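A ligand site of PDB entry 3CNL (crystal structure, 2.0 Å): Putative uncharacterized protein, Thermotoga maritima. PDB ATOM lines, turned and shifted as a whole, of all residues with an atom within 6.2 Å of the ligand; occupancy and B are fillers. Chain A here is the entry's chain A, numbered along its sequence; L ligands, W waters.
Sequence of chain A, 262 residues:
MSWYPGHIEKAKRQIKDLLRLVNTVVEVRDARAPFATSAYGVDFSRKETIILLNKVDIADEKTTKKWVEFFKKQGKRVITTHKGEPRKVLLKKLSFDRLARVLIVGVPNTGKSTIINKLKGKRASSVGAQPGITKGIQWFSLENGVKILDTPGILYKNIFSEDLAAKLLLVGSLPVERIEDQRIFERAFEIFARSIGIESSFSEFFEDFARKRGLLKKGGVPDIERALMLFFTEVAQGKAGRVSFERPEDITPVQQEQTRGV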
ATOM      1  N   VAL A  28      22.200   0.617  20.276  1.00  0.00           N
ATOM      2  CA  VAL A  28      22.490  -0.722  19.778  1.00  0.00           C
ATOM      3  C   VAL A  28      23.962  -1.078  20.035  1.00  0.00           C
ATOM      4  O   VAL A  28      24.885  -0.554  19.363  1.00  0.00           O
ATOM      5  CB  VAL A  28      22.075  -0.900  18.304  1.00  0.00           C
ATOM      6  CG1 VAL A  28      22.367  -2.346  17.787  1.00  0.00           C
ATOM      7  CG2 VAL A  28      20.589  -0.544  18.104  1.00  0.00           C
ATOM      8  N   ASN A  54      22.751  -6.477  21.392  1.00  0.00           N
ATOM      9  CA  ASN A  54      22.414  -7.185  20.165  1.00  0.00           C
ATOM     10  C   ASN A  54      23.330  -8.393  19.919  1.00  0.00           C
ATOM     11  O   ASN A  54      24.349  -8.527  20.571  1.00  0.00           O
ATOM     12  CB  ASN A  54      22.493  -6.199  19.004  1.00  0.00           C
ATOM     13  CG  ASN A  54      21.710  -6.641  17.825  1.00  0.00           C
ATOM     14  OD1 ASN A  54      20.751  -7.363  17.962  1.00  0.00           O
ATOM     15  ND2 ASN A  54      22.100  -6.192  16.637  1.00  0.00           N
ATOM     16  N   LYS A  55      22.974  -9.236  18.949  1.00  0.00           N
ATOM     17  CA  LYS A  55      23.783 -10.389  18.497  1.00  0.00           C
ATOM     18  C   LYS A  55      24.002 -11.440  19.601  1.00  0.00           C
ATOM     19  O   LYS A  55      25.056 -12.106  19.626  1.00  0.00           O
ATOM     20  CB  LYS A  55      25.143  -9.946  17.902  1.00  0.00           C
ATOM     21  CG  LYS A  55      25.055  -8.919  16.741  1.00  0.00           C
ATOM     22  CD  LYS A  55      26.409  -8.666  16.062  1.00  0.00           C
ATOM     23  CE  LYS A  55      26.269  -7.569  15.003  1.00  0.00           C
ATOM     24  NZ  LYS A  55      27.541  -7.361  14.258  1.00  0.00           N
ATOM     25  N   VAL A  56      23.013 -11.636  20.495  1.00  0.00           N
ATOM     26  CA  VAL A  56      23.156 -12.618  21.601  1.00  0.00           C
ATOM     27  C   VAL A  56      23.359 -14.047  21.081  1.00  0.00           C
ATOM     28  O   VAL A  56      23.882 -14.961  21.792  1.00  0.00           O
ATOM     29  CB  VAL A  56      21.981 -12.555  22.649  1.00  0.00           C
ATOM     30  CG1 VAL A  56      21.962 -11.201  23.364  1.00  0.00           C
ATOM     31  CG2 VAL A  56      20.627 -12.906  22.013  1.00  0.00           C
ATOM     32  N   ASP A  57      22.999 -14.244  19.821  1.00  0.00           N
ATOM     33  CA  ASP A  57      23.122 -15.558  19.192  1.00  0.00           C
ATOM     34  C   ASP A  57      24.571 -16.016  18.994  1.00  0.00           C
ATOM     35  O   ASP A  57      24.854 -17.218  18.969  1.00  0.00           O
ATOM     36  CB  ASP A  57      22.337 -15.601  17.889  1.00  0.00           C
ATOM     37  CG  ASP A  57      22.867 -14.626  16.864  1.00  0.00           C
ATOM     38  OD1 ASP A  57      23.008 -13.445  17.222  1.00  0.00           O
ATOM     39  OD2 ASP A  57      23.145 -15.033  15.717  1.00  0.00           O
ATOM     40  N   ILE A  58      25.502 -15.057  18.910  1.00  0.00           N
ATOM     41  CA  ILE A  58      26.934 -15.349  18.740  1.00  0.00           C
ATOM     42  C   ILE A  58      27.759 -14.935  19.972  1.00  0.00           C
ATOM     43  O   ILE A  58      29.003 -14.972  19.943  1.00  0.00           O
ATOM     44  CB  ILE A  58      27.505 -14.734  17.433  1.00  0.00           C
ATOM     45  CG1 ILE A  58      27.313 -13.201  17.366  1.00  0.00           C
ATOM     46  CG2 ILE A  58      26.890 -15.430  16.192  1.00  0.00           C
ATOM     47  CD1 ILE A  58      27.878 -12.564  16.137  1.00  0.00           C
ATOM     48  N   THR A  81      18.641  -8.973  22.285  1.00  0.00           N
ATOM     49  CA  THR A  81      17.967  -9.470  21.100  1.00  0.00           C
ATOM     50  C   THR A  81      18.979  -9.966  20.092  1.00  0.00           C
ATOM     51  O   THR A  81      20.171  -9.950  20.359  1.00  0.00           O
ATOM     52  CB  THR A  81      17.071  -8.381  20.457  1.00  0.00           C
ATOM     53  OG1 THR A  81      16.217  -9.001  19.469  1.00  0.00           O
ATOM     54  CG2 THR A  81      17.913  -7.293  19.778  1.00  0.00           C
ATOM     55  N   HIS A  82      18.482 -10.450  18.957  1.00  0.00           N
ATOM     56  CA  HIS A  82      19.330 -10.880  17.849  1.00  0.00           C
ATOM     57  C   HIS A  82      18.511 -10.864  16.565  1.00  0.00           C
ATOM     58  O   HIS A  82      17.290 -10.777  16.596  1.00  0.00           O
ATOM     59  CB  HIS A  82      19.974 -12.253  18.127  1.00  0.00           C
ATOM     60  CG  HIS A  82      19.033 -13.420  18.051  1.00  0.00           C
ATOM     61  ND1 HIS A  82      18.335 -13.888  19.142  1.00  0.00           N
ATOM     62  CD2 HIS A  82      18.708 -14.230  17.019  1.00  0.00           C
ATOM     63  CE1 HIS A  82      17.605 -14.930  18.780  1.00  0.00           C
ATOM     64  NE2 HIS A  82      17.807 -15.154  17.502  1.00  0.00           N
ATOM     65  N   LYS A  83      19.229 -10.885  15.440  1.00  0.00           N
ATOM     66  CA  LYS A  83      18.711 -10.856  14.060  1.00  0.00           C
ATOM     67  C   LYS A  83      17.481 -11.737  13.850  1.00  0.00           C
ATOM     68  O   LYS A  83      16.527 -11.362  13.162  1.00  0.00           O
ATOM     69  CB  LYS A  83      19.835 -11.433  13.189  1.00  0.00           C
ATOM     70  CG  LYS A  83      20.096 -10.811  11.877  1.00  0.00           C
ATOM     71  CD  LYS A  83      21.229 -11.585  11.209  1.00  0.00           C
ATOM     72  CE  LYS A  83      21.835 -10.820  10.045  1.00  0.00           C
ATOM     73  NZ  LYS A  83      22.956 -11.600   9.374  1.00  0.00           N
ATOM     74  N   GLY A  84      17.541 -12.941  14.431  1.00  0.00           N
ATOM     75  CA  GLY A  84      16.563 -13.986  14.159  1.00  0.00           C
ATOM     76  C   GLY A  84      15.369 -14.021  15.091  1.00  0.00           C
ATOM     77  O   GLY A  84      14.494 -14.883  14.945  1.00  0.00           O
ATOM     78  N   GLY A 106      24.358   3.909  17.504  1.00  0.00           N
ATOM     79  CA  GLY A 106      25.421   2.979  17.934  1.00  0.00           C
ATOM     80  C   GLY A 106      26.705   3.137  17.141  1.00  0.00           C
ATOM     81  O   GLY A 106      26.750   3.858  16.138  1.00  0.00           O
ATOM     82  N   VAL A 107      27.754   2.441  17.577  1.00  0.00           N
ATOM     83  CA  VAL A 107      29.014   2.486  16.817  1.00  0.00           C
ATOM     84  C   VAL A 107      28.815   1.619  15.588  1.00  0.00           C
ATOM     85  O   VAL A 107      27.821   0.903  15.527  1.00  0.00           O
ATOM     86  CB  VAL A 107      30.202   2.009  17.654  1.00  0.00           C
ATOM     87  CG1 VAL A 107      30.365   2.881  18.919  1.00  0.00           C
ATOM     88  CG2 VAL A 107      30.062   0.492  18.011  1.00  0.00           C
ATOM     89  N   PRO A 108      29.727   1.677  14.602  1.00  0.00           N
ATOM     90  CA  PRO A 108      29.569   0.870  13.413  1.00  0.00           C
ATOM     91  C   PRO A 108      29.424  -0.628  13.691  1.00  0.00           C
ATOM     92  O   PRO A 108      30.025  -1.144  14.646  1.00  0.00           O
ATOM     93  CB  PRO A 108      30.873   1.135  12.652  1.00  0.00           C
ATOM     94  CG  PRO A 108      31.318   2.487  13.105  1.00  0.00           C
ATOM     95  CD  PRO A 108      30.938   2.532  14.552  1.00  0.00           C
ATOM     96  N   ASN A 109      28.594  -1.284  12.875  1.00  0.00           N
ATOM     97  CA  ASN A 109      28.507  -2.747  12.743  1.00  0.00           C
ATOM     98  C   ASN A 109      27.656  -3.497  13.750  1.00  0.00           C
ATOM     99  O   ASN A 109      27.520  -4.721  13.661  1.00  0.00           O
ATOM    100  CB  ASN A 109      29.919  -3.392  12.687  1.00  0.00           C
ATOM    101  CG  ASN A 109      29.905  -4.738  12.021  1.00  0.00           C
ATOM    102  OD1 ASN A 109      29.409  -4.858  10.924  1.00  0.00           O
ATOM    103  ND2 ASN A 109      30.435  -5.779  12.702  1.00  0.00           N
ATOM    104  N   THR A 110      27.066  -2.777  14.699  1.00  0.00           N
ATOM    105  CA  THR A 110      26.379  -3.441  15.849  1.00  0.00           C
ATOM    106  C   THR A 110      24.995  -3.987  15.507  1.00  0.00           C
ATOM    107  O   THR A 110      24.390  -4.656  16.339  1.00  0.00           O
ATOM    108  CB  THR A 110      26.205  -2.502  17.028  1.00  0.00           C
ATOM    109  OG1 THR A 110      25.457  -1.345  16.598  1.00  0.00           O
ATOM    110  CG2 THR A 110      27.559  -2.065  17.584  1.00  0.00           C
ATOM    111  N   GLY A 111      24.490  -3.673  14.314  1.00  0.00           N
ATOM    112  CA  GLY A 111      23.221  -4.268  13.835  1.00  0.00           C
ATOM    113  C   GLY A 111      22.063  -3.292  13.630  1.00  0.00           C
ATOM    114  O   GLY A 111      20.906  -3.715  13.594  1.00  0.00           O
ATOM    115  N   LYS A 112      22.378  -2.004  13.458  1.00  0.00           N
ATOM    116  CA  LYS A 112      21.362  -0.946  13.462  1.00  0.00           C
ATOM    117  C   LYS A 112      20.439  -0.968  12.249  1.00  0.00           C
ATOM    118  O   LYS A 112      19.215  -0.786  12.395  1.00  0.00           O
ATOM    119  CB  LYS A 112      22.032   0.426  13.620  1.00  0.00           C
ATOM    120  CG  LYS A 112      22.929   0.537  14.856  1.00  0.00           C
ATOM    121  CD  LYS A 112      23.648   1.887  14.958  1.00  0.00           C
ATOM    122  CE  LYS A 112      24.566   2.153  13.786  1.00  0.00           C
ATOM    123  NZ  LYS A 112      25.597   1.098  13.650  1.00  0.00           N
ATOM    124  N   SER A 113      21.016  -1.194  11.067  1.00  0.00           N
ATOM    125  CA  SER A 113      20.251  -1.269   9.815  1.00  0.00           C
ATOM    126  C   SER A 113      19.337  -2.487   9.803  1.00  0.00           C
ATOM    127  O   SER A 113      18.181  -2.400   9.375  1.00  0.00           O
ATOM    128  CB  SER A 113      21.198  -1.342   8.629  1.00  0.00           C
ATOM    129  OG  SER A 113      21.959  -0.148   8.552  1.00  0.00           O
ATOM    130  N   THR A 114      19.860  -3.593  10.317  1.00  0.00           N
ATOM    131  CA  THR A 114      19.118  -4.832  10.472  1.00  0.00           C
ATOM    132  C   THR A 114      17.917  -4.645  11.404  1.00  0.00           C
ATOM    133  O   THR A 114      16.810  -5.093  11.087  1.00  0.00           O
ATOM    134  CB  THR A 114      20.069  -5.946  10.944  1.00  0.00           C
ATOM    135  OG1 THR A 114      21.118  -6.097   9.964  1.00  0.00           O
ATOM    136  CG2 THR A 114      19.336  -7.293  11.123  1.00  0.00           C
ATOM    137  N   ILE A 115      18.124  -3.989  12.538  1.00  0.00           N
ATOM    138  CA  ILE A 115      17.025  -3.685  13.473  1.00  0.00           C
ATOM    139  C   ILE A 115      15.935  -2.796  12.843  1.00  0.00           C
ATOM    140  O   ILE A 115      14.740  -3.083  12.977  1.00  0.00           O
ATOM    141  CB  ILE A 115      17.581  -3.106  14.801  1.00  0.00           C
ATOM    142  CG1 ILE A 115      18.312  -4.218  15.568  1.00  0.00           C
ATOM    143  CG2 ILE A 115      16.470  -2.477  15.675  1.00  0.00           C
ATOM    144  CD1 ILE A 115      19.072  -3.756  16.768  1.00  0.00           C
ATOM    145  N   PRO A 152      19.815   5.209  11.109  1.00  0.00           N
ATOM    146  CA  PRO A 152      20.462   5.235  12.415  1.00  0.00           C
ATOM    147  C   PRO A 152      21.503   6.340  12.504  1.00  0.00           C
ATOM    148  O   PRO A 152      22.020   6.798  11.476  1.00  0.00           O
ATOM    149  CB  PRO A 152      21.143   3.869  12.494  1.00  0.00           C
ATOM    150  CG  PRO A 152      21.444   3.517  11.106  1.00  0.00           C
ATOM    151  CD  PRO A 152      20.364   4.142  10.254  1.00  0.00           C
ATOM    152  N   ILE A 154      25.272   7.037  13.563  1.00  0.00           N
ATOM    153  CA  ILE A 154      26.458   6.215  13.699  1.00  0.00           C
ATOM    154  C   ILE A 154      27.456   6.978  14.568  1.00  0.00           C
ATOM    155  O   ILE A 154      27.828   8.108  14.260  1.00  0.00           O
ATOM    156  CB  ILE A 154      27.063   5.864  12.331  1.00  0.00           C
ATOM    157  CG1 ILE A 154      26.027   5.161  11.459  1.00  0.00           C
ATOM    158  CG2 ILE A 154      28.339   5.016  12.487  1.00  0.00           C
ATOM    159  CD1 ILE A 154      26.374   5.083   9.984  1.00  0.00           C
ATOM    160  N   ALA A 236      34.153 -11.431  14.205  1.00  0.00           N
ATOM    161  CA  ALA A 236      33.108 -10.406  14.293  1.00  0.00           C
ATOM    162  C   ALA A 236      31.733 -10.964  13.877  1.00  0.00           C
ATOM    163  O   ALA A 236      30.698 -10.556  14.404  1.00  0.00           O
ATOM    164  CB  ALA A 236      33.473  -9.255  13.414  1.00  0.00           C
ATOM    165  N   GLN A 237      31.770 -11.903  12.923  1.00  0.00           N
ATOM    166  CA  GLN A 237      30.605 -12.593  12.384  1.00  0.00           C
ATOM    167  C   GLN A 237      30.145 -13.785  13.243  1.00  0.00           C
ATOM    168  O   GLN A 237      29.120 -14.381  12.962  1.00  0.00           O
ATOM    169  CB  GLN A 237      30.896 -13.043  10.946  1.00  0.00           C
ATOM    170  CG  GLN A 237      31.121 -11.864   9.981  1.00  0.00           C
ATOM    171  CD  GLN A 237      31.609 -12.270   8.609  1.00  0.00           C
ATOM    172  OE1 GLN A 237      32.194 -13.341   8.434  1.00  0.00           O
ATOM    173  NE2 GLN A 237      31.402 -11.395   7.617  1.00  0.00           N
ATOM    174  N   GLY A 238      30.890 -14.104  14.297  1.00  0.00           N
ATOM    175  CA  GLY A 238      30.535 -15.239  15.139  1.00  0.00           C
ATOM    176  C   GLY A 238      30.922 -16.590  14.534  1.00  0.00           C
ATOM    177  O   GLY A 238      30.446 -17.632  14.988  1.00  0.00           O
HETATM  178  P1  LIG L   1      26.958   0.247  10.210  1.00  0.00           P
HETATM  179  O1  LIG L   1      26.462   1.416  11.038  1.00  0.00           O
HETATM  180  O2  LIG L   1      28.451   0.009  10.403  1.00  0.00           O
HETATM  181  O3  LIG L   1      26.531   0.465   8.767  1.00  0.00           O
HETATM  182  N1  LIG L   1      26.331  -1.180  10.482  1.00  0.00           N
HETATM  183  P2  LIG L   1      24.997  -1.533  11.256  1.00  0.00           P
HETATM  184  O4  LIG L   1      25.119  -1.129  12.690  1.00  0.00           O
HETATM  185  O5  LIG L   1      23.847  -0.946  10.497  1.00  0.00           O
HETATM  186  O6  LIG L   1      24.912  -3.070  11.200  1.00  0.00           O
HETATM  187  P3  LIG L   1      24.213  -4.000  10.155  1.00  0.00           P
HETATM  188  O7  LIG L   1      22.791  -4.173  10.482  1.00  0.00           O
HETATM  189  O8  LIG L   1      24.537  -3.629   8.772  1.00  0.00           O
HETATM  190  O9  LIG L   1      24.857  -5.387  10.459  1.00  0.00           O
HETATM  191  C1  LIG L   1      26.273  -5.605  10.428  1.00  0.00           C
HETATM  192  C2  LIG L   1      26.521  -7.094  10.281  1.00  0.00           C
HETATM  193  O10 LIG L   1      26.056  -7.839  11.455  1.00  0.00           O
HETATM  194  C3  LIG L   1      25.834  -7.781   9.112  1.00  0.00           C
HETATM  195  O11 LIG L   1      26.704  -8.792   8.619  1.00  0.00           O
HETATM  196  C4  LIG L   1      24.615  -8.400   9.762  1.00  0.00           C
HETATM  197  O12 LIG L   1      24.151  -9.503   9.009  1.00  0.00           O
HETATM  198  C5  LIG L   1      25.164  -8.874  11.109  1.00  0.00           C
HETATM  199  N2  LIG L   1      24.193  -8.925  12.188  1.00  0.00           N
HETATM  200  C6  LIG L   1      23.286  -7.939  12.524  1.00  0.00           C
HETATM  201  N3  LIG L   1      22.557  -8.262  13.576  1.00  0.00           N
HETATM  202  C7  LIG L   1      23.014  -9.547  13.933  1.00  0.00           C
HETATM  203  C8  LIG L   1      22.627 -10.418  14.987  1.00  0.00           C
HETATM  204  O13 LIG L   1      21.757 -10.240  15.845  1.00  0.00           O
HETATM  205  N4  LIG L   1      23.371 -11.613  14.984  1.00  0.00           N
HETATM  206  C9  LIG L   1      24.379 -11.927  14.079  1.00  0.00           C
HETATM  207  N5  LIG L   1      24.987 -13.119  14.225  1.00  0.00           N
HETATM  208  N6  LIG L   1      24.761 -11.118  13.106  1.00  0.00           N
HETATM  209  C10 LIG L   1      24.038  -9.956  13.092  1.00  0.00           C
HETATM  210  O   HOH W   1      24.017   2.005  10.134  1.00  0.00           O
HETATM  211  O   HOH W   2      30.424  -1.175   9.545  1.00  0.00           O
HETATM  212  O   HOH W   3      28.569  -9.562  13.097  1.00  0.00           O
HETATM  213  O   HOH W   4      24.725  -1.028   7.471  1.00  0.00           O
HETATM  214  O   HOH W   5      21.472  -8.038   8.403  1.00  0.00           O
HETATM  215  O   HOH W   6      20.487  -6.392  14.310  1.00  0.00           O
HETATM  216  O   HOH W   7      28.398  -2.734   9.213  1.00  0.00           O
HETATM  217  O   HOH W   8      27.276 -11.569  11.997  1.00  0.00           O
HETATM  218  O   HOH W   9      26.699 -14.443  12.044  1.00  0.00           O
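O of Val 107 lies within hydrogen-bond range of NZ of Lys 112 (2.9 Å). O of Asn 109 lies within hydrogen-bond range of NZ of Lys 55, at 2.7 Å. O of Thr 81 is in hydrogen-bond range of N of Lys 55 (3.2 Å). The backbone carbonyl oxygen (O) of Thr 110 is in hydrogen-bond range of the side-chain amide nitrogen (ND2) of Asn 54, 2.8 Å away. The side-chain hydroxyl of Thr 110 sits at hydrogen-bond distance from the backbone carbonyl oxygen of Val 107 (3.4 Å). The backbone carbonyl oxygen of Val 28 lies within hydrogen-bond range of the side-chain hydroxyl of Thr 110 (2.9 Å).
Water W1 bridges an oxygen (O1) of the ligand and the side-chain hydroxyl (OG) of Ser 113. Water W4 bridges O3 of the ligand (2.7 Å) and OG of Ser 113 (3.1 Å). Water W7 lies within hydrogen-bond range of N1 of the ligand (2.9 Å) and OD1 of Asn 109 (2.9 Å). Water W6 lies within hydrogen-bond range of the backbone carbonyl oxygen of Gly 111 (2.8 Å), the side-chain amide nitrogen of Asn 54 (2.8 Å) and a nitrogen (N3) of the ligand (2.9 Å). Water W9 lies within hydrogen-bond range of O of Gln 237 and N5 of the ligand. Water W3 lies within hydrogen-bond range of O of Ala 236, NZ of Lys 55 and O10 of the ligand.
Merely in contact with the ligand: Asn 54, Ile 58, His 82, Pro 108 and Ile 154. Of the 25 residues printed, 14 come within 4 Å of the ligand.
N of Lys 83 lies within hydrogen-bond range of O13 of the ligand (2.6 Å). NZ of Lys 83 lies within hydrogen-bond range of O12 of the ligand, at 2.4 Å. The backbone NH (N) of Lys 112 is in hydrogen-bond range of an oxygen (O4) of the ligand (3.0 Å). The side-chain amino group (NZ) of Lys 112 is in salt-bridge range of an oxygen (O4) of the ligand, at 2.5 Å. An oxygen (O7) of the ligand lies within hydrogen-bond range of the backbone NH of Thr 114 (3.0 Å). An oxygen (O7) of the ligand sits at hydrogen-bond distance from the side-chain hydroxyl (OG1) of Thr 114 (2.6 Å). N of Asn 109 lies within hydrogen-bond range of O2 of the ligand (2.8 Å). O5 of the ligand is in hydrogen-bond range of N of Ser 113 (2.9 Å). An oxygen (O5) of the ligand is in hydrogen-bond range of the side-chain hydroxyl (OG) of Ser 113. The side-chain carboxylate of Asp 57 sits at hydrogen-bond distance from a nitrogen (N4) of the ligand, at 2.9 Å. An oxygen (O4) of the ligand sits at hydrogen-bond distance from the backbone NH of Gly 111, 3.1 Å away. The backbone NH (N) of Lys 55 lies close to an oxygen (O13) of the ligand, 3.5 Å away. The side-chain amino group (NZ) of Lys 55 is in hydrogen-bond range of an oxygen (O10) of the ligand, 3.2 Å away. O4 of the ligand sits at hydrogen-bond distance from N of Thr 110.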
